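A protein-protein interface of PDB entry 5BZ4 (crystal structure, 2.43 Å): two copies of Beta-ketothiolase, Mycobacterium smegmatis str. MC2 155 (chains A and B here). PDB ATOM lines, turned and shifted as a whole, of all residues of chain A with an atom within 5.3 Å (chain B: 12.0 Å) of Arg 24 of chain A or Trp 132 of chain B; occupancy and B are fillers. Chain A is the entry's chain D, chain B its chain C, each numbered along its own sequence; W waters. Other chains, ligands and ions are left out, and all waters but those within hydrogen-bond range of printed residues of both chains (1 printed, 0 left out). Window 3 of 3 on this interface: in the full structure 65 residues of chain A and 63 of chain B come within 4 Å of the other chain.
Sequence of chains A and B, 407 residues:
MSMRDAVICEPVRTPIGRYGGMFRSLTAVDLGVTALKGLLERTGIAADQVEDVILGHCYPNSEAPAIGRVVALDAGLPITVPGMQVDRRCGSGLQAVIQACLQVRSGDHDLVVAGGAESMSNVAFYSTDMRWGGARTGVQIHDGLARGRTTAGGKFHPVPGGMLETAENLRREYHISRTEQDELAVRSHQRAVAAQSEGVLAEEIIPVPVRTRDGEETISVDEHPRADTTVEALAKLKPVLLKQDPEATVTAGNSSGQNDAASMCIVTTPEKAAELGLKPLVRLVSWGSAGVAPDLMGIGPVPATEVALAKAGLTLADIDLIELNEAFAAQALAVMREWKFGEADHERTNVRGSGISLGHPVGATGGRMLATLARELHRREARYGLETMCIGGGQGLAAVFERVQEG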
ATOM      1  N   TYR A  19       1.517 -17.109 -29.470  1.00  0.00           N
ATOM      2  CA  TYR A  19       2.735 -16.483 -29.941  1.00  0.00           C
ATOM      3  C   TYR A  19       2.364 -15.145 -30.588  1.00  0.00           C
ATOM      4  O   TYR A  19       1.628 -15.119 -31.581  1.00  0.00           O
ATOM      5  CB  TYR A  19       3.420 -17.428 -30.926  1.00  0.00           C
ATOM      6  CG  TYR A  19       4.644 -16.934 -31.679  1.00  0.00           C
ATOM      7  CD1 TYR A  19       5.855 -16.736 -31.037  1.00  0.00           C
ATOM      8  CD2 TYR A  19       4.598 -16.740 -33.056  1.00  0.00           C
ATOM      9  CE1 TYR A  19       6.963 -16.325 -31.735  1.00  0.00           C
ATOM     10  CE2 TYR A  19       5.709 -16.321 -33.765  1.00  0.00           C
ATOM     11  CZ  TYR A  19       6.884 -16.117 -33.098  1.00  0.00           C
ATOM     12  OH  TYR A  19       7.995 -15.711 -33.790  1.00  0.00           O
ATOM     13  N   GLY A  20       2.832 -14.042 -30.005  1.00  0.00           N
ATOM     14  CA  GLY A  20       2.538 -12.717 -30.516  1.00  0.00           C
ATOM     15  C   GLY A  20       1.173 -12.217 -30.076  1.00  0.00           C
ATOM     16  O   GLY A  20       0.622 -11.253 -30.648  1.00  0.00           O
ATOM     17  N   GLY A  21       0.638 -12.858 -29.039  1.00  0.00           N
ATOM     18  CA  GLY A  21      -0.734 -12.647 -28.626  1.00  0.00           C
ATOM     19  C   GLY A  21      -0.886 -11.878 -27.337  1.00  0.00           C
ATOM     20  O   GLY A  21      -0.226 -10.854 -27.143  1.00  0.00           O
ATOM     21  N   MET A  22      -1.753 -12.374 -26.455  1.00  0.00           N
ATOM     22  CA  MET A  22      -2.183 -11.616 -25.283  1.00  0.00           C
ATOM     23  C   MET A  22      -1.037 -11.302 -24.339  1.00  0.00           C
ATOM     24  O   MET A  22      -1.102 -10.343 -23.575  1.00  0.00           O
ATOM     25  CB  MET A  22      -3.295 -12.372 -24.545  1.00  0.00           C
ATOM     26  CG  MET A  22      -2.846 -13.549 -23.700  1.00  0.00           C
ATOM     27  SD  MET A  22      -4.265 -14.591 -23.300  1.00  0.00           S
ATOM     28  CE  MET A  22      -3.540 -15.821 -22.232  1.00  0.00           C
ATOM     29  N   PHE A  23       0.031 -12.083 -24.430  1.00  0.00           N
ATOM     30  CA  PHE A  23       1.124 -11.956 -23.483  1.00  0.00           C
ATOM     31  C   PHE A  23       2.411 -11.436 -24.123  1.00  0.00           C
ATOM     32  O   PHE A  23       3.442 -11.343 -23.458  1.00  0.00           O
ATOM     33  CB  PHE A  23       1.382 -13.309 -22.790  1.00  0.00           C
ATOM     34  CG  PHE A  23       0.356 -13.675 -21.726  1.00  0.00           C
ATOM     35  CD1 PHE A  23      -0.390 -12.699 -21.086  1.00  0.00           C
ATOM     36  CD2 PHE A  23       0.193 -14.992 -21.327  1.00  0.00           C
ATOM     37  CE1 PHE A  23      -1.309 -13.034 -20.090  1.00  0.00           C
ATOM     38  CE2 PHE A  23      -0.719 -15.332 -20.333  1.00  0.00           C
ATOM     39  CZ  PHE A  23      -1.475 -14.346 -19.719  1.00  0.00           C
ATOM     40  N   ARG A  24       2.346 -11.073 -25.398  1.00  0.00           N
ATOM     41  CA  ARG A  24       3.522 -10.613 -26.131  1.00  0.00           C
ATOM     42  C   ARG A  24       4.265  -9.489 -25.421  1.00  0.00           C
ATOM     43  O   ARG A  24       5.422  -9.224 -25.733  1.00  0.00           O
ATOM     44  CB  ARG A  24       3.119 -10.144 -27.520  1.00  0.00           C
ATOM     45  CG  ARG A  24       4.258  -9.923 -28.495  1.00  0.00           C
ATOM     46  CD  ARG A  24       3.697  -9.441 -29.820  1.00  0.00           C
ATOM     47  NE  ARG A  24       4.178  -8.102 -30.147  1.00  0.00           N
ATOM     48  CZ  ARG A  24       3.794  -7.391 -31.207  1.00  0.00           C
ATOM     49  NH1 ARG A  24       2.907  -7.871 -32.078  1.00  0.00           N
ATOM     50  NH2 ARG A  24       4.309  -6.185 -31.398  1.00  0.00           N
ATOM     51  N   SER A  25       3.601  -8.844 -24.464  1.00  0.00           N
ATOM     52  CA  SER A  25       4.193  -7.757 -23.690  1.00  0.00           C
ATOM     53  C   SER A  25       5.066  -8.255 -22.539  1.00  0.00           C
ATOM     54  O   SER A  25       5.901  -7.516 -22.023  1.00  0.00           O
ATOM     55  CB  SER A  25       3.088  -6.829 -23.141  1.00  0.00           C
ATOM     56  OG  SER A  25       1.980  -7.532 -22.594  1.00  0.00           O
ATOM     57  N   LEU A  26       4.870  -9.502 -22.123  1.00  0.00           N
ATOM     58  CA  LEU A  26       5.526  -9.977 -20.908  1.00  0.00           C
ATOM     59  C   LEU A  26       6.675 -10.915 -21.202  1.00  0.00           C
ATOM     60  O   LEU A  26       6.581 -11.784 -22.076  1.00  0.00           O
ATOM     61  CB  LEU A  26       4.524 -10.677 -19.980  1.00  0.00           C
ATOM     62  CG  LEU A  26       3.235  -9.971 -19.562  1.00  0.00           C
ATOM     63  CD1 LEU A  26       2.482 -10.838 -18.571  1.00  0.00           C
ATOM     64  CD2 LEU A  26       3.520  -8.597 -18.977  1.00  0.00           C
ATOM     65  N   SER A 121       7.006 -15.646 -27.584  1.00  0.00           N
ATOM     66  CA  SER A 121       6.842 -14.383 -28.314  1.00  0.00           C
ATOM     67  C   SER A 121       8.098 -13.527 -28.272  1.00  0.00           C
ATOM     68  O   SER A 121       8.279 -12.667 -29.107  1.00  0.00           O
ATOM     69  CB  SER A 121       5.676 -13.564 -27.743  1.00  0.00           C
ATOM     70  OG  SER A 121       4.453 -14.263 -27.805  1.00  0.00           O
ATOM     71  N   ASN A 122       8.961 -13.757 -27.291  1.00  0.00           N
ATOM     72  CA  ASN A 122      10.120 -12.897 -27.116  1.00  0.00           C
ATOM     73  C   ASN A 122      11.449 -13.629 -27.109  1.00  0.00           C
ATOM     74  O   ASN A 122      12.455 -13.100 -26.625  1.00  0.00           O
ATOM     75  CB  ASN A 122       9.972 -12.091 -25.832  1.00  0.00           C
ATOM     76  CG  ASN A 122       8.919 -11.025 -25.946  1.00  0.00           C
ATOM     77  OD1 ASN A 122       7.967 -10.991 -25.176  1.00  0.00           O
ATOM     78  ND2 ASN A 122       9.083 -10.139 -26.920  1.00  0.00           N
ATOM     79  N   ASP A 260       3.122 -18.610 -24.718  1.00  0.00           N
ATOM     80  CA  ASP A 260       3.753 -18.011 -23.552  1.00  0.00           C
ATOM     81  C   ASP A 260       3.004 -18.422 -22.268  1.00  0.00           C
ATOM     82  O   ASP A 260       1.771 -18.321 -22.195  1.00  0.00           O
ATOM     83  CB  ASP A 260       3.780 -16.475 -23.659  1.00  0.00           C
ATOM     84  CG  ASP A 260       4.253 -15.962 -25.016  1.00  0.00           C
ATOM     85  OD1 ASP A 260       5.289 -16.417 -25.540  1.00  0.00           O
ATOM     86  OD2 ASP A 260       3.587 -15.060 -25.553  1.00  0.00           O
ATOM     87  N   SER B 127      19.226 -10.170 -29.875  1.00  0.00           N
ATOM     88  CA  SER B 127      18.294  -9.068 -29.825  1.00  0.00           C
ATOM     89  C   SER B 127      16.897  -9.561 -29.557  1.00  0.00           C
ATOM     90  O   SER B 127      16.468 -10.593 -30.072  1.00  0.00           O
ATOM     91  CB  SER B 127      18.323  -8.263 -31.129  1.00  0.00           C
ATOM     92  OG  SER B 127      17.460  -7.147 -31.063  1.00  0.00           O
ATOM     93  N   THR B 128      16.179  -8.796 -28.755  1.00  0.00           N
ATOM     94  CA  THR B 128      14.782  -9.085 -28.523  1.00  0.00           C
ATOM     95  C   THR B 128      13.883  -8.184 -29.382  1.00  0.00           C
ATOM     96  O   THR B 128      12.675  -8.172 -29.202  1.00  0.00           O
ATOM     97  CB  THR B 128      14.458  -8.943 -27.025  1.00  0.00           C
ATOM     98  OG1 THR B 128      14.904  -7.668 -26.553  1.00  0.00           O
ATOM     99  CG2 THR B 128      15.192 -10.019 -26.249  1.00  0.00           C
ATOM    100  N   ASP B 129      14.481  -7.457 -30.329  1.00  0.00           N
ATOM    101  CA  ASP B 129      13.747  -6.506 -31.166  1.00  0.00           C
ATOM    102  C   ASP B 129      13.556  -6.874 -32.638  1.00  0.00           C
ATOM    103  O   ASP B 129      13.024  -6.074 -33.393  1.00  0.00           O
ATOM    104  CB  ASP B 129      14.431  -5.141 -31.126  1.00  0.00           C
ATOM    105  CG  ASP B 129      14.580  -4.616 -29.739  1.00  0.00           C
ATOM    106  OD1 ASP B 129      13.557  -4.602 -29.033  1.00  0.00           O
ATOM    107  OD2 ASP B 129      15.706  -4.214 -29.371  1.00  0.00           O
ATOM    108  N   MET B 130      13.972  -8.057 -33.063  1.00  0.00           N
ATOM    109  CA  MET B 130      13.877  -8.382 -34.479  1.00  0.00           C
ATOM    110  C   MET B 130      12.648  -9.175 -34.877  1.00  0.00           C
ATOM    111  O   MET B 130      12.283  -9.211 -36.047  1.00  0.00           O
ATOM    112  CB  MET B 130      15.139  -9.135 -34.910  1.00  0.00           C
ATOM    113  CG  MET B 130      16.385  -8.339 -34.644  1.00  0.00           C
ATOM    114  SD  MET B 130      17.853  -9.209 -35.143  1.00  0.00           S
ATOM    115  CE  MET B 130      19.057  -7.980 -34.702  1.00  0.00           C
ATOM    116  N   ARG B 131      11.997  -9.799 -33.906  1.00  0.00           N
ATOM    117  CA  ARG B 131      10.897 -10.719 -34.185  1.00  0.00           C
ATOM    118  C   ARG B 131       9.652  -9.987 -34.660  1.00  0.00           C
ATOM    119  O   ARG B 131       8.927 -10.466 -35.538  1.00  0.00           O
ATOM    120  CB  ARG B 131      10.567 -11.556 -32.933  1.00  0.00           C
ATOM    121  CG  ARG B 131       9.646 -12.734 -33.179  1.00  0.00           C
ATOM    122  CD  ARG B 131       9.529 -13.626 -31.948  1.00  0.00           C
ATOM    123  NE  ARG B 131      10.778 -14.320 -31.627  1.00  0.00           N
ATOM    124  CZ  ARG B 131      11.301 -15.317 -32.339  1.00  0.00           C
ATOM    125  NH1 ARG B 131      10.698 -15.753 -33.437  1.00  0.00           N
ATOM    126  NH2 ARG B 131      12.435 -15.878 -31.954  1.00  0.00           N
ATOM    127  N   TRP B 132       9.421  -8.817 -34.075  1.00  0.00           N
ATOM    128  CA  TRP B 132       8.223  -8.054 -34.351  1.00  0.00           C
ATOM    129  C   TRP B 132       8.549  -6.751 -35.040  1.00  0.00           C
ATOM    130  O   TRP B 132       7.648  -6.073 -35.537  1.00  0.00           O
ATOM    131  CB  TRP B 132       7.444  -7.816 -33.057  1.00  0.00           C
ATOM    132  CG  TRP B 132       7.194  -9.096 -32.321  1.00  0.00           C
ATOM    133  CD1 TRP B 132       7.710  -9.469 -31.116  1.00  0.00           C
ATOM    134  CD2 TRP B 132       6.404 -10.208 -32.786  1.00  0.00           C
ATOM    135  NE1 TRP B 132       7.269 -10.728 -30.784  1.00  0.00           N
ATOM    136  CE2 TRP B 132       6.481 -11.198 -31.776  1.00  0.00           C
ATOM    137  CE3 TRP B 132       5.653 -10.441 -33.931  1.00  0.00           C
ATOM    138  CZ2 TRP B 132       5.801 -12.428 -31.908  1.00  0.00           C
ATOM    139  CZ3 TRP B 132       4.991 -11.651 -34.052  1.00  0.00           C
ATOM    140  CH2 TRP B 132       5.067 -12.632 -33.041  1.00  0.00           C
ATOM    141  N   GLY B 133       9.837  -6.413 -35.078  1.00  0.00           N
ATOM    142  CA  GLY B 133      10.318  -5.277 -35.844  1.00  0.00           C
ATOM    143  C   GLY B 133      10.698  -4.068 -35.005  1.00  0.00           C
ATOM    144  O   GLY B 133       9.998  -3.744 -34.035  1.00  0.00           O
ATOM    145  N   GLY B 134      11.794  -3.396 -35.376  1.00  0.00           N
ATOM    146  CA  GLY B 134      12.212  -2.187 -34.686  1.00  0.00           C
ATOM    147  C   GLY B 134      11.667  -0.884 -35.257  1.00  0.00           C
ATOM    148  O   GLY B 134      12.213   0.184 -34.988  1.00  0.00           O
ATOM    149  N   ALA B 135      10.584  -0.980 -36.028  1.00  0.00           N
ATOM    150  CA  ALA B 135       9.957   0.179 -36.683  1.00  0.00           C
ATOM    151  C   ALA B 135       9.822   1.419 -35.795  1.00  0.00           C
ATOM    152  O   ALA B 135       9.994   2.540 -36.270  1.00  0.00           O
ATOM    153  CB  ALA B 135       8.576  -0.211 -37.220  1.00  0.00           C
ATOM    154  N   ARG B 136       9.505   1.214 -34.515  1.00  0.00           N
ATOM    155  CA  ARG B 136       9.301   2.325 -33.586  1.00  0.00           C
ATOM    156  C   ARG B 136      10.332   2.397 -32.464  1.00  0.00           C
ATOM    157  O   ARG B 136      10.648   3.485 -31.982  1.00  0.00           O
ATOM    158  CB  ARG B 136       7.903   2.240 -32.971  1.00  0.00           C
ATOM    159  N   THR B 137      10.850   1.241 -32.051  1.00  0.00           N
ATOM    160  CA  THR B 137      11.722   1.144 -30.874  1.00  0.00           C
ATOM    161  C   THR B 137      13.203   1.126 -31.206  1.00  0.00           C
ATOM    162  O   THR B 137      14.031   1.340 -30.320  1.00  0.00           O
ATOM    163  CB  THR B 137      11.447  -0.139 -30.073  1.00  0.00           C
ATOM    164  OG1 THR B 137      11.960  -1.248 -30.809  1.00  0.00           O
ATOM    165  CG2 THR B 137       9.963  -0.336 -29.879  1.00  0.00           C
ATOM    166  N   GLY B 138      13.531   0.836 -32.465  1.00  0.00           N
ATOM    167  CA  GLY B 138      14.903   0.519 -32.831  1.00  0.00           C
ATOM    168  C   GLY B 138      15.245  -0.944 -32.557  1.00  0.00           C
ATOM    169  O   GLY B 138      14.392  -1.710 -32.132  1.00  0.00           O
ATOM    170  N   VAL B 139      16.488  -1.324 -32.818  1.00  0.00           N
ATOM    171  CA  VAL B 139      16.983  -2.670 -32.559  1.00  0.00           C
ATOM    172  C   VAL B 139      18.247  -2.639 -31.712  1.00  0.00           C
ATOM    173  O   VAL B 139      19.315  -2.319 -32.210  1.00  0.00           O
ATOM    174  CB  VAL B 139      17.292  -3.423 -33.867  1.00  0.00           C
ATOM    175  CG1 VAL B 139      17.886  -4.785 -33.567  1.00  0.00           C
ATOM    176  CG2 VAL B 139      16.033  -3.543 -34.710  1.00  0.00           C
ATOM    177  N   GLN B 140      18.118  -2.983 -30.438  1.00  0.00           N
ATOM    178  CA  GLN B 140      19.276  -3.169 -29.579  1.00  0.00           C
ATOM    179  C   GLN B 140      19.830  -4.585 -29.710  1.00  0.00           C
ATOM    180  O   GLN B 140      19.068  -5.544 -29.661  1.00  0.00           O
ATOM    181  CB  GLN B 140      18.902  -2.882 -28.132  1.00  0.00           C
ATOM    182  CG  GLN B 140      20.050  -2.432 -27.276  1.00  0.00           C
ATOM    183  CD  GLN B 140      19.607  -2.088 -25.864  1.00  0.00           C
ATOM    184  OE1 GLN B 140      18.406  -1.944 -25.591  1.00  0.00           O
ATOM    185  NE2 GLN B 140      20.575  -1.969 -24.949  1.00  0.00           N
HETATM  186  O   HOH W   1      10.644 -10.105 -28.790  1.00  0.00           O
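The guanidinium group (NH1) of Arg 131 of chain B lies within hydrogen-bond range of the side-chain hydroxyl (OH) of Tyr 19 of chain A (2.7 Å). NE1 of Trp 132 of chain B lies within hydrogen-bond range of O of Ser 121 of chain A (2.8 Å).
The side-chain hydroxyl (OG) of Ser 121 of chain A lies within hydrogen-bond range of the side-chain carboxylate (OD2) of Asp 260 of chain A (2.5 Å). The backbone carbonyl oxygen (O) of Arg 24 of chain A sits close to the side-chain amide oxygen (OD1) of Asn 122 of chain A (3.1 Å). The backbone NH (N) of Gly 20 of chain A sits at hydrogen-bond distance from the side-chain hydroxyl (OG) of Ser 121 of chain A (2.7 Å).
Trp 132 of chain B touches Tyr 19 of chain A (CH2 to CE2, 3.8 Å). Gly 20 of chain A touches Trp 132 of chain B. Trp 132 of chain B touches Arg 24 of chain A (CE2 to CD, 3.8 Å). Ser 121 of chain A touches Arg 131 of chain B (O to CD, 3.2 Å).
Of chain B, only Trp 132 (3.8 Å) comes within 4 Å of Arg 24 of chain A. Trp 132 of chain B touches four residues of chain A. No residue of chain B comes within 4 Å of Gly 21 of chain A. No residue of chain B comes within 4 Å of Phe 23 of chain A. Ser 25 of chain A touches none of the printed residues of chain B. No residue of chain B comes within 4 Å of Leu 26 of chain A. Of chain B, only Arg 131 (3.2 Å) and Trp 132 (2.8 Å) come within 4 Å of Ser 121 of chain A. Printed residues of chain A within 4 Å of Arg 131 of chain B: Tyr 19 (2.7 Å) and Ser 121 (3.2 Å). The nearest residue of chain B that does not touch Arg 24 of chain A is Gly 133 of chain B (6.6 Å). The nearest residue of chain A that does not touch Trp 132 of chain B is Asn 122 of chain A (4.3 Å).
Printed residues of chain A that touch a printed residue of chain B: Tyr 19, Gly 20, Arg 24 and Ser 121. Hydrophobic or aromatic side chains of chain A that line the printed part of chain B: Tyr 19. Hydrophobic or aromatic side chains of chain B within 4 Å of the printed part of chain A: Trp 132.
No position is printed for both chains. Of the 6 pairs that touch across the chains among the printed residues, none has its exchanged pair printed and touching as well.
Water W1 bridges the side-chain amide nitrogen of Asn 122 of chain A (2.4 Å) and the backbone carbonyl oxygen of Thr 128 of chain B (2.8 Å).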
